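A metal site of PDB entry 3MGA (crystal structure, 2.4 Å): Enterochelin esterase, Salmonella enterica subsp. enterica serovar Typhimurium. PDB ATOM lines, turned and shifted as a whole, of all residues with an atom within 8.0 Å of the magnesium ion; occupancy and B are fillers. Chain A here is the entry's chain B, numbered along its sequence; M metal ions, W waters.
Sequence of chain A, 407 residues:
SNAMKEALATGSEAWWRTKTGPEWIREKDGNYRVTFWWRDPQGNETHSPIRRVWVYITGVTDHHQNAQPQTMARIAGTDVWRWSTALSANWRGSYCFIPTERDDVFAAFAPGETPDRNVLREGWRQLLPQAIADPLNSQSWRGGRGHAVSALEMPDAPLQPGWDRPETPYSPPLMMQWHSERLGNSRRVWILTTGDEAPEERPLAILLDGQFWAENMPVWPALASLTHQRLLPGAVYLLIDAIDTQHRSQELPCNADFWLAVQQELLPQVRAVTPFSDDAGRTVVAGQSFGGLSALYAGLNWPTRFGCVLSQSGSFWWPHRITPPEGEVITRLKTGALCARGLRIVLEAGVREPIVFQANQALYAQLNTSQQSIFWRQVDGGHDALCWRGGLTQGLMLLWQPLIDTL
The side-chain hydroxyl of Thr 323 lies close to the backbone carbonyl oxygen of His 320 (3.5 Å).
Four residues have an atom within 4 Å of the magnesium ion: Trp 317, His 320, Thr 323 and Glu 326.
The magnesium ion is bound by O of Glu 326, O of Trp 317, O of Thr 323 and O of His 320. Slightly farther from the magnesium ion lies water W1 (2.7 Å).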
ATOM      1  N   SER A 315     -21.396  24.210 -21.868  1.00  0.00           N
ATOM      2  CA  SER A 315     -22.102  24.381 -20.597  1.00  0.00           C
ATOM      3  C   SER A 315     -21.629  25.629 -19.854  1.00  0.00           C
ATOM      4  O   SER A 315     -21.137  25.552 -18.736  1.00  0.00           O
ATOM      5  CB  SER A 315     -21.898  23.141 -19.716  1.00  0.00           C
ATOM      6  OG  SER A 315     -22.482  22.005 -20.331  1.00  0.00           O
ATOM      7  N   PHE A 316     -21.826  26.793 -20.474  1.00  0.00           N
ATOM      8  CA  PHE A 316     -21.358  28.041 -19.887  1.00  0.00           C
ATOM      9  C   PHE A 316     -22.219  28.555 -18.729  1.00  0.00           C
ATOM     10  O   PHE A 316     -21.931  29.616 -18.158  1.00  0.00           O
ATOM     11  CB  PHE A 316     -21.132  29.079 -20.969  1.00  0.00           C
ATOM     12  CG  PHE A 316     -20.095  28.638 -21.961  1.00  0.00           C
ATOM     13  CD1 PHE A 316     -18.753  28.653 -21.610  1.00  0.00           C
ATOM     14  CD2 PHE A 316     -20.455  28.198 -23.217  1.00  0.00           C
ATOM     15  CE1 PHE A 316     -17.790  28.238 -22.508  1.00  0.00           C
ATOM     16  CE2 PHE A 316     -19.503  27.785 -24.105  1.00  0.00           C
ATOM     17  CZ  PHE A 316     -18.166  27.794 -23.748  1.00  0.00           C
ATOM     18  N   TRP A 317     -23.239  27.777 -18.383  1.00  0.00           N
ATOM     19  CA  TRP A 317     -24.095  28.045 -17.246  1.00  0.00           C
ATOM     20  C   TRP A 317     -23.392  27.602 -15.958  1.00  0.00           C
ATOM     21  O   TRP A 317     -23.764  28.015 -14.865  1.00  0.00           O
ATOM     22  CB  TRP A 317     -25.430  27.285 -17.382  1.00  0.00           C
ATOM     23  CG  TRP A 317     -25.264  25.835 -17.721  1.00  0.00           C
ATOM     24  CD1 TRP A 317     -25.443  25.268 -18.951  1.00  0.00           C
ATOM     25  CD2 TRP A 317     -24.845  24.768 -16.857  1.00  0.00           C
ATOM     26  NE1 TRP A 317     -25.183  23.924 -18.902  1.00  0.00           N
ATOM     27  CE2 TRP A 317     -24.819  23.592 -17.631  1.00  0.00           C
ATOM     28  CE3 TRP A 317     -24.519  24.693 -15.496  1.00  0.00           C
ATOM     29  CZ2 TRP A 317     -24.455  22.349 -17.096  1.00  0.00           C
ATOM     30  CZ3 TRP A 317     -24.160  23.464 -14.969  1.00  0.00           C
ATOM     31  CH2 TRP A 317     -24.140  22.308 -15.765  1.00  0.00           C
ATOM     32  N   TRP A 318     -22.374  26.753 -16.116  1.00  0.00           N
ATOM     33  CA  TRP A 318     -21.628  26.197 -14.977  1.00  0.00           C
ATOM     34  C   TRP A 318     -21.080  27.289 -14.061  1.00  0.00           C
ATOM     35  O   TRP A 318     -20.605  28.313 -14.546  1.00  0.00           O
ATOM     36  CB  TRP A 318     -20.501  25.291 -15.502  1.00  0.00           C
ATOM     37  CG  TRP A 318     -19.801  24.503 -14.445  1.00  0.00           C
ATOM     38  CD1 TRP A 318     -20.163  23.271 -13.969  1.00  0.00           C
ATOM     39  CD2 TRP A 318     -18.626  24.882 -13.736  1.00  0.00           C
ATOM     40  NE1 TRP A 318     -19.280  22.873 -13.004  1.00  0.00           N
ATOM     41  CE2 TRP A 318     -18.318  23.839 -12.839  1.00  0.00           C
ATOM     42  CE3 TRP A 318     -17.800  26.009 -13.770  1.00  0.00           C
ATOM     43  CZ2 TRP A 318     -17.219  23.884 -11.985  1.00  0.00           C
ATOM     44  CZ3 TRP A 318     -16.702  26.060 -12.929  1.00  0.00           C
ATOM     45  CH2 TRP A 318     -16.421  24.998 -12.047  1.00  0.00           C
ATOM     46  N   PRO A 319     -21.084  27.057 -12.740  1.00  0.00           N
ATOM     47  CA  PRO A 319     -21.487  25.875 -11.957  1.00  0.00           C
ATOM     48  C   PRO A 319     -22.985  25.542 -11.808  1.00  0.00           C
ATOM     49  O   PRO A 319     -23.336  24.366 -11.759  1.00  0.00           O
ATOM     50  CB  PRO A 319     -20.893  26.170 -10.578  1.00  0.00           C
ATOM     51  CG  PRO A 319     -20.933  27.631 -10.475  1.00  0.00           C
ATOM     52  CD  PRO A 319     -20.661  28.161 -11.858  1.00  0.00           C
ATOM     53  N   HIS A 320     -23.844  26.550 -11.725  1.00  0.00           N
ATOM     54  CA  HIS A 320     -25.269  26.279 -11.520  1.00  0.00           C
ATOM     55  C   HIS A 320     -26.177  26.446 -12.746  1.00  0.00           C
ATOM     56  O   HIS A 320     -26.287  27.525 -13.324  1.00  0.00           O
ATOM     57  CB  HIS A 320     -25.799  27.113 -10.348  1.00  0.00           C
ATOM     58  CG  HIS A 320     -25.006  26.948  -9.100  1.00  0.00           C
ATOM     59  ND1 HIS A 320     -25.008  25.783  -8.368  1.00  0.00           N
ATOM     60  CD2 HIS A 320     -24.173  27.800  -8.442  1.00  0.00           C
ATOM     61  CE1 HIS A 320     -24.215  25.914  -7.318  1.00  0.00           C
ATOM     62  NE2 HIS A 320     -23.698  27.130  -7.342  1.00  0.00           N
ATOM     63  N   ARG A 321     -26.827  25.344 -13.100  1.00  0.00           N
ATOM     64  CA  ARG A 321     -27.762  25.309 -14.223  1.00  0.00           C
ATOM     65  C   ARG A 321     -29.061  26.027 -13.854  1.00  0.00           C
ATOM     66  O   ARG A 321     -29.825  26.441 -14.723  1.00  0.00           O
ATOM     67  CB  ARG A 321     -28.042  23.838 -14.604  1.00  0.00           C
ATOM     68  CG  ARG A 321     -29.029  23.644 -15.736  1.00  0.00           C
ATOM     69  CD  ARG A 321     -29.220  22.155 -16.035  1.00  0.00           C
ATOM     70  NE  ARG A 321     -28.011  21.544 -16.592  1.00  0.00           N
ATOM     71  CZ  ARG A 321     -27.895  20.240 -16.884  1.00  0.00           C
ATOM     72  NH1 ARG A 321     -28.894  19.405 -16.651  1.00  0.00           N
ATOM     73  NH2 ARG A 321     -26.754  19.778 -17.391  1.00  0.00           N
ATOM     74  N   ILE A 322     -29.302  26.181 -12.545  1.00  0.00           N
ATOM     75  CA  ILE A 322     -30.490  26.869 -12.047  1.00  0.00           C
ATOM     76  C   ILE A 322     -30.583  28.290 -12.623  1.00  0.00           C
ATOM     77  O   ILE A 322     -31.666  28.818 -12.813  1.00  0.00           O
ATOM     78  CB  ILE A 322     -30.500  26.927 -10.490  1.00  0.00           C
ATOM     79  CG1 ILE A 322     -31.847  27.402  -9.957  1.00  0.00           C
ATOM     80  CG2 ILE A 322     -29.347  27.803  -9.985  1.00  0.00           C
ATOM     81  CD1 ILE A 322     -33.010  26.492 -10.305  1.00  0.00           C
ATOM     82  N   THR A 323     -29.418  28.889 -12.873  1.00  0.00           N
ATOM     83  CA  THR A 323     -29.326  30.221 -13.468  1.00  0.00           C
ATOM     84  C   THR A 323     -28.571  30.068 -14.796  1.00  0.00           C
ATOM     85  O   THR A 323     -27.338  30.095 -14.816  1.00  0.00           O
ATOM     86  CB  THR A 323     -28.576  31.196 -12.547  1.00  0.00           C
ATOM     87  OG1 THR A 323     -27.260  30.683 -12.283  1.00  0.00           O
ATOM     88  CG2 THR A 323     -29.328  31.384 -11.234  1.00  0.00           C
ATOM     89  N   PRO A 324     -29.302  29.874 -15.902  1.00  0.00           N
ATOM     90  CA  PRO A 324     -28.688  29.666 -17.225  1.00  0.00           C
ATOM     91  C   PRO A 324     -27.700  30.741 -17.728  1.00  0.00           C
ATOM     92  O   PRO A 324     -26.631  30.382 -18.223  1.00  0.00           O
ATOM     93  CB  PRO A 324     -29.892  29.575 -18.173  1.00  0.00           C
ATOM     94  CG  PRO A 324     -31.042  29.192 -17.316  1.00  0.00           C
ATOM     95  CD  PRO A 324     -30.778  29.754 -15.960  1.00  0.00           C
ATOM     96  N   PRO A 325     -28.046  32.041 -17.606  1.00  0.00           N
ATOM     97  CA  PRO A 325     -27.169  33.097 -18.144  1.00  0.00           C
ATOM     98  C   PRO A 325     -26.009  33.561 -17.246  1.00  0.00           C
ATOM     99  O   PRO A 325     -25.291  34.505 -17.602  1.00  0.00           O
ATOM    100  CB  PRO A 325     -28.149  34.259 -18.381  1.00  0.00           C
ATOM    101  CG  PRO A 325     -29.228  34.067 -17.330  1.00  0.00           C
ATOM    102  CD  PRO A 325     -29.201  32.618 -16.896  1.00  0.00           C
ATOM    103  N   GLU A 326     -25.823  32.918 -16.088  1.00  0.00           N
ATOM    104  CA  GLU A 326     -24.737  33.269 -15.192  1.00  0.00           C
ATOM    105  C   GLU A 326     -23.777  32.086 -15.111  1.00  0.00           C
ATOM    106  O   GLU A 326     -24.213  30.945 -15.026  1.00  0.00           O
ATOM    107  CB  GLU A 326     -25.277  33.618 -13.800  1.00  0.00           C
ATOM    108  CG  GLU A 326     -26.296  34.736 -13.814  1.00  0.00           C
ATOM    109  CD  GLU A 326     -26.828  35.074 -12.442  1.00  0.00           C
ATOM    110  OE1 GLU A 326     -26.162  34.772 -11.430  1.00  0.00           O
ATOM    111  OE2 GLU A 326     -27.932  35.660 -12.371  1.00  0.00           O
ATOM    112  N   GLY A 327     -22.476  32.376 -15.137  1.00  0.00           N
ATOM    113  CA  GLY A 327     -21.463  31.337 -15.064  1.00  0.00           C
ATOM    114  C   GLY A 327     -20.047  31.846 -14.908  1.00  0.00           C
ATOM    115  O   GLY A 327     -19.735  32.983 -15.246  1.00  0.00           O
ATOM    116  N   GLU A 328     -19.184  30.977 -14.388  1.00  0.00           N
ATOM    117  CA  GLU A 328     -17.770  31.278 -14.165  1.00  0.00           C
ATOM    118  C   GLU A 328     -17.130  32.027 -15.341  1.00  0.00           C
ATOM    119  O   GLU A 328     -16.692  33.169 -15.199  1.00  0.00           O
ATOM    120  CB  GLU A 328     -17.009  29.975 -13.880  1.00  0.00           C
ATOM    121  CG  GLU A 328     -15.498  30.103 -13.625  1.00  0.00           C
ATOM    122  CD  GLU A 328     -15.162  30.822 -12.333  1.00  0.00           C
ATOM    123  OE1 GLU A 328     -16.067  31.071 -11.515  1.00  0.00           O
ATOM    124  OE2 GLU A 328     -13.956  31.118 -12.125  1.00  0.00           O
ATOM    125  N   ILE A 330     -18.416  33.443 -17.910  1.00  0.00           N
ATOM    126  CA  ILE A 330     -19.124  34.669 -18.257  1.00  0.00           C
ATOM    127  C   ILE A 330     -18.684  35.818 -17.324  1.00  0.00           C
ATOM    128  O   ILE A 330     -18.519  36.956 -17.772  1.00  0.00           O
ATOM    129  CB  ILE A 330     -20.666  34.477 -18.189  1.00  0.00           C
ATOM    130  CG1 ILE A 330     -21.130  33.475 -19.247  1.00  0.00           C
ATOM    131  CG2 ILE A 330     -21.391  35.805 -18.385  1.00  0.00           C
ATOM    132  CD1 ILE A 330     -22.625  33.200 -19.235  1.00  0.00           C
ATOM    133  N   ILE A 355     -31.791  26.074 -22.122  1.00  0.00           N
ATOM    134  CA  ILE A 355     -30.886  26.507 -21.062  1.00  0.00           C
ATOM    135  C   ILE A 355     -29.481  26.702 -21.613  1.00  0.00           C
ATOM    136  O   ILE A 355     -28.822  27.704 -21.322  1.00  0.00           O
ATOM    137  CB  ILE A 355     -30.862  25.505 -19.881  1.00  0.00           C
ATOM    138  CG1 ILE A 355     -32.282  25.290 -19.331  1.00  0.00           C
ATOM    139  CG2 ILE A 355     -29.928  25.996 -18.780  1.00  0.00           C
ATOM    140  CD1 ILE A 355     -32.372  24.258 -18.237  1.00  0.00           C
ATOM    141  N   ALA A 359     -27.447  30.255 -22.120  1.00  0.00           N
ATOM    142  CA  ALA A 359     -26.117  30.397 -21.513  1.00  0.00           C
ATOM    143  C   ALA A 359     -25.107  30.857 -22.554  1.00  0.00           C
ATOM    144  O   ALA A 359     -24.279  31.710 -22.255  1.00  0.00           O
ATOM    145  CB  ALA A 359     -25.666  29.097 -20.868  1.00  0.00           C
HETATM  146 MG    MG M   1     -25.394  29.309 -14.219  1.00  0.00          MG
HETATM  147  O   HOH W   1     -23.837  29.583 -12.025  1.00  0.00           O
